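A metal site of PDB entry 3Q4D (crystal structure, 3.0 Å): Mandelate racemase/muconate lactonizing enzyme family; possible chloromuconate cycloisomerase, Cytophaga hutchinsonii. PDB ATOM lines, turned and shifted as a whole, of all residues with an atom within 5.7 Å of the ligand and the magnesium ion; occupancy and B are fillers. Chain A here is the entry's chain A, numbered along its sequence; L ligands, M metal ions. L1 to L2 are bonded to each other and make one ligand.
N1 of LG2 L2 lies within hydrogen-bond range of O of Gly 293 (2.8 Å).
A nitrogen (N1) of LIG L1 lies within salt-bridge range of the side-chain carboxylate of Asp 318 (2.6 Å).
The side-chain amino group (NZ) of Lys 265 is in salt-bridge range of an oxygen (O1) of LG2 L2, 2.5 Å away.
NZ of Lys 162 is in hydrogen-bond range of O1 of LIG L1 (3.1 Å).
The side-chain amino group (NZ) of Lys 160 lies within salt-bridge range of an oxygen (O1) of LG2 L2 (3.0 Å).
OD1 of Asn 192 lies close to O2 of LG2 L2 (3.5 Å).
The side-chain carboxylate (OD1) of Asp 320 lies within salt-bridge range of a nitrogen (N1) of LIG L1, at 2.7 Å.
OG1 of Thr 135 lies within hydrogen-bond range of N1 of LIG L1 (2.9 Å).
The side-chain carboxylate of Glu 216 sits close to the side-chain amide nitrogen of Asn 263.
The side-chain amino group (NZ) of Lys 162 lies close to the side-chain amide nitrogen (ND2) of Asn 192.
The side-chain carboxylate (OD2) of Asp 318 sits close to the side-chain carboxylate (OD2) of Asp 133 (2.5 Å).
The side-chain carboxylate (OD1) of Asp 190 is in hydrogen-bond range of the backbone NH (N) of Asn 192, 3.0 Å away.
N of Thr 135 lies within hydrogen-bond range of OD2 of Asp 320 (2.7 Å).
The side-chain amino group (NZ) of Lys 265 lies close to the side-chain carboxylate (OD2) of Asp 241, 3.5 Å away.
The side-chain carboxylate of Glu 216 is in salt-bridge range of the side-chain amino group of Lys 160, 2.9 Å away.
OG1 of Thr 321 lies within hydrogen-bond range of O of Phe 294.
Phe 19 touches the ligand.
O of Phe 294 touches C2 of LIG L1, at 3.6 Å.
CG2 of Thr 321 touches C1 of LIG L1, at 3.6 Å.
Hydrophobic or aromatic side chains within 4 Å of the ligand: Phe 19.
Within 4 Å of the ligand: Phe 19, Thr 135, Lys 160, Lys 162, Asp 190, Asn 192, Glu 216, Asp 241, Lys 265, Gly 293, Phe 294, Asp 318, Asp 320 and Thr 321.
Along chain A the residues within 4 Å of the ligand span positions 19 to 321.
The nearest printed residue that does not touch the ligand is Phe 51 (4.05 Å).
Merely in contact with the magnesium ion: Lys 160 and Asn 263.
Within 4 Å of the magnesium ion: Lys 160, Asp 190, Glu 216, Asp 241 and Asn 263.
Along chain A the residues within 4 Å of the magnesium ion span positions 160 to 263.
The nearest printed residue that does not touch the magnesium ion is Asn 192 (4.01 Å).
The magnesium ion is bound by the side-chain carboxylate of Asp 241 (2.0 Å), the side-chain carboxylate of Glu 216 (2.2 Å), the side-chain carboxylate of Asp 190 (2.3 Å) and an oxygen (O2) of LG2 L2 (2.5 Å).
The magnesium ion has four donor atoms within binding distance.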
ATOM      1  N   PHE A  19      32.837  11.061  -2.471  1.00  0.00           N
ATOM      2  CA  PHE A  19      31.836  11.622  -1.590  1.00  0.00           C
ATOM      3  C   PHE A  19      32.516  12.566  -0.623  1.00  0.00           C
ATOM      4  O   PHE A  19      33.528  12.207  -0.025  1.00  0.00           O
ATOM      5  CB  PHE A  19      31.158  10.478  -0.823  1.00  0.00           C
ATOM      6  CG  PHE A  19      30.016  10.894   0.057  1.00  0.00           C
ATOM      7  CD1 PHE A  19      28.810  11.283  -0.492  1.00  0.00           C
ATOM      8  CD2 PHE A  19      30.122  10.832   1.429  1.00  0.00           C
ATOM      9  CE1 PHE A  19      27.737  11.631   0.329  1.00  0.00           C
ATOM     10  CE2 PHE A  19      29.065  11.166   2.248  1.00  0.00           C
ATOM     11  CZ  PHE A  19      27.871  11.574   1.699  1.00  0.00           C
ATOM     12  N   ILE A  21      32.154  15.526   2.463  1.00  0.00           N
ATOM     13  CA  ILE A  21      31.464  16.259   3.516  1.00  0.00           C
ATOM     14  C   ILE A  21      32.468  17.156   4.231  1.00  0.00           C
ATOM     15  O   ILE A  21      33.656  17.051   4.005  1.00  0.00           O
ATOM     16  CB  ILE A  21      30.785  15.313   4.533  1.00  0.00           C
ATOM     17  CG1 ILE A  21      31.818  14.376   5.159  1.00  0.00           C
ATOM     18  CG2 ILE A  21      29.707  14.528   3.889  1.00  0.00           C
ATOM     19  CD1 ILE A  21      31.251  13.507   6.248  1.00  0.00           C
ATOM     20  N   PHE A  51      32.406   4.922   9.239  1.00  0.00           N
ATOM     21  CA  PHE A  51      32.854   6.250   8.889  1.00  0.00           C
ATOM     22  C   PHE A  51      33.821   6.733   9.962  1.00  0.00           C
ATOM     23  O   PHE A  51      33.397   7.138  11.023  1.00  0.00           O
ATOM     24  CB  PHE A  51      31.660   7.167   8.903  1.00  0.00           C
ATOM     25  CG  PHE A  51      31.400   7.871   7.626  1.00  0.00           C
ATOM     26  CD1 PHE A  51      31.721   9.210   7.488  1.00  0.00           C
ATOM     27  CD2 PHE A  51      30.776   7.217   6.575  1.00  0.00           C
ATOM     28  CE1 PHE A  51      31.435   9.886   6.312  1.00  0.00           C
ATOM     29  CE2 PHE A  51      30.488   7.899   5.392  1.00  0.00           C
ATOM     30  CZ  PHE A  51      30.826   9.228   5.267  1.00  0.00           C
ATOM     31  N   ILE A  54      33.044   9.853  12.226  1.00  0.00           N
ATOM     32  CA  ILE A  54      31.783   9.910  12.954  1.00  0.00           C
ATOM     33  C   ILE A  54      31.567   8.722  13.879  1.00  0.00           C
ATOM     34  O   ILE A  54      31.233   8.898  15.060  1.00  0.00           O
ATOM     35  CB  ILE A  54      30.590  10.060  12.016  1.00  0.00           C
ATOM     36  CG1 ILE A  54      30.769  11.291  11.136  1.00  0.00           C
ATOM     37  CG2 ILE A  54      29.287  10.122  12.812  1.00  0.00           C
ATOM     38  CD1 ILE A  54      29.591  11.562  10.251  1.00  0.00           C
ATOM     39  N   ASP A 133      16.035  11.925  -0.924  1.00  0.00           N
ATOM     40  CA  ASP A 133      16.720  13.054  -1.482  1.00  0.00           C
ATOM     41  C   ASP A 133      17.907  12.514  -2.238  1.00  0.00           C
ATOM     42  O   ASP A 133      18.083  11.306  -2.334  1.00  0.00           O
ATOM     43  CB  ASP A 133      17.170  13.991  -0.355  1.00  0.00           C
ATOM     44  CG  ASP A 133      18.003  13.293   0.723  1.00  0.00           C
ATOM     45  OD1 ASP A 133      17.769  13.567   1.904  1.00  0.00           O
ATOM     46  OD2 ASP A 133      18.906  12.488   0.392  1.00  0.00           O
ATOM     47  N   THR A 135      22.270  13.638  -2.525  1.00  0.00           N
ATOM     48  CA  THR A 135      23.265  14.481  -1.891  1.00  0.00           C
ATOM     49  C   THR A 135      24.230  15.134  -2.864  1.00  0.00           C
ATOM     50  O   THR A 135      24.824  14.477  -3.714  1.00  0.00           O
ATOM     51  CB  THR A 135      24.070  13.675  -0.839  1.00  0.00           C
ATOM     52  OG1 THR A 135      23.198  13.242   0.194  1.00  0.00           O
ATOM     53  CG2 THR A 135      25.155  14.503  -0.201  1.00  0.00           C
ATOM     54  N   LYS A 160      19.782  17.184  -0.987  1.00  0.00           N
ATOM     55  CA  LYS A 160      20.527  17.392   0.251  1.00  0.00           C
ATOM     56  C   LYS A 160      21.901  17.984  -0.042  1.00  0.00           C
ATOM     57  O   LYS A 160      22.691  17.388  -0.751  1.00  0.00           O
ATOM     58  CB  LYS A 160      20.652  16.082   1.027  1.00  0.00           C
ATOM     59  CG  LYS A 160      21.499  16.160   2.264  1.00  0.00           C
ATOM     60  CD  LYS A 160      21.221  14.981   3.173  1.00  0.00           C
ATOM     61  CE  LYS A 160      22.247  14.869   4.264  1.00  0.00           C
ATOM     62  NZ  LYS A 160      21.990  13.714   5.146  1.00  0.00           N
ATOM     63  N   LYS A 162      25.615  19.452   1.148  1.00  0.00           N
ATOM     64  CA  LYS A 162      26.628  19.423   2.192  1.00  0.00           C
ATOM     65  C   LYS A 162      27.304  20.793   2.324  1.00  0.00           C
ATOM     66  O   LYS A 162      27.991  21.262   1.421  1.00  0.00           O
ATOM     67  CB  LYS A 162      27.655  18.322   1.931  1.00  0.00           C
ATOM     68  CG  LYS A 162      27.101  16.920   2.028  1.00  0.00           C
ATOM     69  CD  LYS A 162      26.671  16.600   3.440  1.00  0.00           C
ATOM     70  CE  LYS A 162      26.289  15.162   3.594  1.00  0.00           C
ATOM     71  NZ  LYS A 162      26.014  14.831   5.021  1.00  0.00           N
ATOM     72  N   ASP A 190      23.275  20.151   5.351  1.00  0.00           N
ATOM     73  CA  ASP A 190      23.967  19.336   6.348  1.00  0.00           C
ATOM     74  C   ASP A 190      25.397  19.834   6.488  1.00  0.00           C
ATOM     75  O   ASP A 190      26.166  19.781   5.538  1.00  0.00           O
ATOM     76  CB  ASP A 190      23.943  17.858   5.918  1.00  0.00           C
ATOM     77  CG  ASP A 190      24.444  16.913   7.005  1.00  0.00           C
ATOM     78  OD1 ASP A 190      25.167  17.358   7.928  1.00  0.00           O
ATOM     79  OD2 ASP A 190      24.115  15.723   6.938  1.00  0.00           O
ATOM     80  N   ASN A 192      27.582  18.789   8.972  1.00  0.00           N
ATOM     81  CA  ASN A 192      28.439  17.819   9.645  1.00  0.00           C
ATOM     82  C   ASN A 192      29.384  18.458  10.639  1.00  0.00           C
ATOM     83  O   ASN A 192      30.590  18.264  10.546  1.00  0.00           O
ATOM     84  CB  ASN A 192      29.233  16.982   8.651  1.00  0.00           C
ATOM     85  CG  ASN A 192      28.362  16.028   7.882  1.00  0.00           C
ATOM     86  OD1 ASN A 192      27.772  15.123   8.464  1.00  0.00           O
ATOM     87  ND2 ASN A 192      28.264  16.215   6.568  1.00  0.00           N
ATOM     88  N   GLU A 216      21.088  19.874   9.127  1.00  0.00           N
ATOM     89  CA  GLU A 216      21.598  18.830   9.988  1.00  0.00           C
ATOM     90  C   GLU A 216      22.886  19.254  10.667  1.00  0.00           C
ATOM     91  O   GLU A 216      23.732  19.850  10.046  1.00  0.00           O
ATOM     92  CB  GLU A 216      21.861  17.540   9.216  1.00  0.00           C
ATOM     93  CG  GLU A 216      20.633  16.774   8.782  1.00  0.00           C
ATOM     94  CD  GLU A 216      20.994  15.584   7.894  1.00  0.00           C
ATOM     95  OE1 GLU A 216      21.894  14.820   8.275  1.00  0.00           O
ATOM     96  OE2 GLU A 216      20.364  15.418   6.817  1.00  0.00           O
ATOM     97  N   ASP A 241      22.065  15.095  14.080  1.00  0.00           N
ATOM     98  CA  ASP A 241      22.553  13.855  13.498  1.00  0.00           C
ATOM     99  C   ASP A 241      23.581  13.222  14.434  1.00  0.00           C
ATOM    100  O   ASP A 241      23.218  12.427  15.292  1.00  0.00           O
ATOM    101  CB  ASP A 241      23.143  14.116  12.127  1.00  0.00           C
ATOM    102  CG  ASP A 241      23.261  12.866  11.294  1.00  0.00           C
ATOM    103  OD1 ASP A 241      23.403  11.778  11.878  1.00  0.00           O
ATOM    104  OD2 ASP A 241      23.233  12.978  10.046  1.00  0.00           O
ATOM    105  N   GLU A 242      24.851  13.588  14.275  1.00  0.00           N
ATOM    106  CA  GLU A 242      25.903  13.068  15.152  1.00  0.00           C
ATOM    107  C   GLU A 242      25.558  13.254  16.645  1.00  0.00           C
ATOM    108  O   GLU A 242      25.942  12.467  17.483  1.00  0.00           O
ATOM    109  CB  GLU A 242      27.265  13.723  14.847  1.00  0.00           C
ATOM    110  CG  GLU A 242      27.855  13.380  13.477  1.00  0.00           C
ATOM    111  CD  GLU A 242      27.395  14.300  12.334  1.00  0.00           C
ATOM    112  OE1 GLU A 242      26.184  14.342  12.020  1.00  0.00           O
ATOM    113  OE2 GLU A 242      28.255  14.962  11.736  1.00  0.00           O
ATOM    114  N   ASN A 263      17.885  12.981  12.928  1.00  0.00           N
ATOM    115  CA  ASN A 263      18.304  12.070  11.895  1.00  0.00           C
ATOM    116  C   ASN A 263      18.711  10.701  12.485  1.00  0.00           C
ATOM    117  O   ASN A 263      19.752  10.554  13.139  1.00  0.00           O
ATOM    118  CB  ASN A 263      19.434  12.674  11.074  1.00  0.00           C
ATOM    119  CG  ASN A 263      19.749  11.873   9.829  1.00  0.00           C
ATOM    120  OD1 ASN A 263      19.464  10.683   9.764  1.00  0.00           O
ATOM    121  ND2 ASN A 263      20.345  12.521   8.845  1.00  0.00           N
ATOM    122  N   LYS A 265      19.869   6.845  12.342  1.00  0.00           N
ATOM    123  CA  LYS A 265      20.668   5.912  11.543  1.00  0.00           C
ATOM    124  C   LYS A 265      20.932   4.657  12.353  1.00  0.00           C
ATOM    125  O   LYS A 265      21.351   4.755  13.497  1.00  0.00           O
ATOM    126  CB  LYS A 265      22.016   6.536  11.152  1.00  0.00           C
ATOM    127  CG  LYS A 265      21.968   7.842  10.353  1.00  0.00           C
ATOM    128  CD  LYS A 265      23.372   8.238   9.921  1.00  0.00           C
ATOM    129  CE  LYS A 265      23.527   9.696   9.556  1.00  0.00           C
ATOM    130  NZ  LYS A 265      22.944  10.043   8.222  1.00  0.00           N
ATOM    131  N   GLY A 292      18.298   8.015   7.770  1.00  0.00           N
ATOM    132  CA  GLY A 292      19.431   8.063   6.858  1.00  0.00           C
ATOM    133  C   GLY A 292      20.427   6.938   7.005  1.00  0.00           C
ATOM    134  O   GLY A 292      20.077   5.827   7.333  1.00  0.00           O
ATOM    135  N   GLY A 293      21.693   7.227   6.772  1.00  0.00           N
ATOM    136  CA  GLY A 293      22.725   6.213   6.842  1.00  0.00           C
ATOM    137  C   GLY A 293      24.067   6.714   6.354  1.00  0.00           C
ATOM    138  O   GLY A 293      24.308   7.904   6.247  1.00  0.00           O
ATOM    139  N   PHE A 294      24.973   5.809   6.034  1.00  0.00           N
ATOM    140  CA  PHE A 294      26.277   6.240   5.552  1.00  0.00           C
ATOM    141  C   PHE A 294      26.542   5.742   4.144  1.00  0.00           C
ATOM    142  O   PHE A 294      25.859   6.141   3.231  1.00  0.00           O
ATOM    143  CB  PHE A 294      27.389   5.885   6.544  1.00  0.00           C
ATOM    144  CG  PHE A 294      27.228   6.564   7.873  1.00  0.00           C
ATOM    145  CD1 PHE A 294      27.879   7.760   8.148  1.00  0.00           C
ATOM    146  CD2 PHE A 294      26.412   6.027   8.860  1.00  0.00           C
ATOM    147  CE1 PHE A 294      27.740   8.382   9.347  1.00  0.00           C
ATOM    148  CE2 PHE A 294      26.254   6.644  10.074  1.00  0.00           C
ATOM    149  CZ  PHE A 294      26.918   7.827  10.322  1.00  0.00           C
ATOM    150  N   LEU A 295      27.517   4.868   3.948  1.00  0.00           N
ATOM    151  CA  LEU A 295      27.730   4.303   2.618  1.00  0.00           C
ATOM    152  C   LEU A 295      27.327   2.835   2.505  1.00  0.00           C
ATOM    153  O   LEU A 295      27.859   2.101   1.688  1.00  0.00           O
ATOM    154  CB  LEU A 295      29.175   4.519   2.163  1.00  0.00           C
ATOM    155  CG  LEU A 295      29.467   5.796   1.382  1.00  0.00           C
ATOM    156  CD1 LEU A 295      28.664   6.956   1.879  1.00  0.00           C
ATOM    157  CD2 LEU A 295      30.917   6.137   1.469  1.00  0.00           C
ATOM    158  N   PHE A 301      20.507  -0.167   3.492  1.00  0.00           N
ATOM    159  CA  PHE A 301      19.423   0.772   3.376  1.00  0.00           C
ATOM    160  C   PHE A 301      18.072   0.095   3.282  1.00  0.00           C
ATOM    161  O   PHE A 301      17.034   0.703   3.531  1.00  0.00           O
ATOM    162  CB  PHE A 301      19.649   1.721   2.207  1.00  0.00           C
ATOM    163  CG  PHE A 301      20.546   2.870   2.537  1.00  0.00           C
ATOM    164  CD1 PHE A 301      20.044   3.999   3.152  1.00  0.00           C
ATOM    165  CD2 PHE A 301      21.880   2.818   2.223  1.00  0.00           C
ATOM    166  CE1 PHE A 301      20.889   5.049   3.454  1.00  0.00           C
ATOM    167  CE2 PHE A 301      22.721   3.880   2.510  1.00  0.00           C
ATOM    168  CZ  PHE A 301      22.225   4.986   3.132  1.00  0.00           C
ATOM    169  N   ASP A 318      16.855   9.844   3.587  1.00  0.00           N
ATOM    170  CA  ASP A 318      18.142  10.068   2.932  1.00  0.00           C
ATOM    171  C   ASP A 318      18.729   8.696   2.610  1.00  0.00           C
ATOM    172  O   ASP A 318      19.509   8.154   3.357  1.00  0.00           O
ATOM    173  CB  ASP A 318      19.076  10.856   3.864  1.00  0.00           C
ATOM    174  CG  ASP A 318      20.400  11.183   3.230  1.00  0.00           C
ATOM    175  OD1 ASP A 318      21.424  11.140   3.945  1.00  0.00           O
ATOM    176  OD2 ASP A 318      20.440  11.490   2.027  1.00  0.00           O
ATOM    177  N   PHE A 319      18.313   8.127   1.494  1.00  0.00           N
ATOM    178  CA  PHE A 319      18.729   6.771   1.151  1.00  0.00           C
ATOM    179  C   PHE A 319      19.476   6.741  -0.166  1.00  0.00           C
ATOM    180  O   PHE A 319      19.222   5.865  -0.982  1.00  0.00           O
ATOM    181  CB  PHE A 319      17.511   5.867   1.010  1.00  0.00           C
ATOM    182  CG  PHE A 319      16.795   5.610   2.300  1.00  0.00           C
ATOM    183  CD1 PHE A 319      17.350   5.942   3.516  1.00  0.00           C
ATOM    184  CD2 PHE A 319      15.544   5.002   2.286  1.00  0.00           C
ATOM    185  CE1 PHE A 319      16.667   5.699   4.690  1.00  0.00           C
ATOM    186  CE2 PHE A 319      14.863   4.743   3.459  1.00  0.00           C
ATOM    187  CZ  PHE A 319      15.419   5.099   4.656  1.00  0.00           C
ATOM    188  N   ASP A 320      20.381   7.680  -0.385  1.00  0.00           N
ATOM    189  CA  ASP A 320      20.887   7.949  -1.728  1.00  0.00           C
ATOM    190  C   ASP A 320      22.187   7.239  -2.100  1.00  0.00           C
ATOM    191  O   ASP A 320      22.368   6.842  -3.235  1.00  0.00           O
ATOM    192  CB  ASP A 320      21.002   9.449  -1.957  1.00  0.00           C
ATOM    193  CG  ASP A 320      22.057  10.109  -1.093  1.00  0.00           C
ATOM    194  OD1 ASP A 320      22.319   9.633   0.038  1.00  0.00           O
ATOM    195  OD2 ASP A 320      22.638  11.120  -1.549  1.00  0.00           O
ATOM    196  N   THR A 321      23.069   7.067  -1.137  1.00  0.00           N
ATOM    197  CA  THR A 321      24.422   6.623  -1.428  1.00  0.00           C
ATOM    198  C   THR A 321      24.605   5.336  -2.255  1.00  0.00           C
ATOM    199  O   THR A 321      25.585   5.210  -2.953  1.00  0.00           O
ATOM    200  CB  THR A 321      25.256   6.508  -0.145  1.00  0.00           C
ATOM    201  OG1 THR A 321      24.491   5.859   0.870  1.00  0.00           O
ATOM    202  CG2 THR A 321      25.631   7.868   0.333  1.00  0.00           C
HETATM  203  N1  LIG L   1      23.234  11.013   2.114  1.00  0.00           N
HETATM  204  C1  LIG L   1      24.240  10.158   2.749  1.00  0.00           C
HETATM  205  C2  LIG L   1      23.604   8.895   3.240  1.00  0.00           C
HETATM  206  C3  LIG L   1      24.916  10.903   3.871  1.00  0.00           C
HETATM  207  O1  LIG L   1      25.147  12.088   3.791  1.00  0.00           O
HETATM  208  N1  LG2 L   2      25.290  10.174   4.929  1.00  0.00           N
HETATM  209  C1  LG2 L   2      25.924  10.754   6.127  1.00  0.00           C
HETATM  210  C2  LG2 L   2      25.047  11.888   6.583  1.00  0.00           C
HETATM  211  O1  LG2 L   2      23.821  11.809   6.607  1.00  0.00           O
HETATM  212  C3  LG2 L   2      27.356  11.230   5.857  1.00  0.00           C
HETATM  213  O2  LG2 L   2      25.557  12.946   6.928  1.00  0.00           O
HETATM  214 MG    MG M   1      23.934  13.974   8.475  1.00  0.00          MG
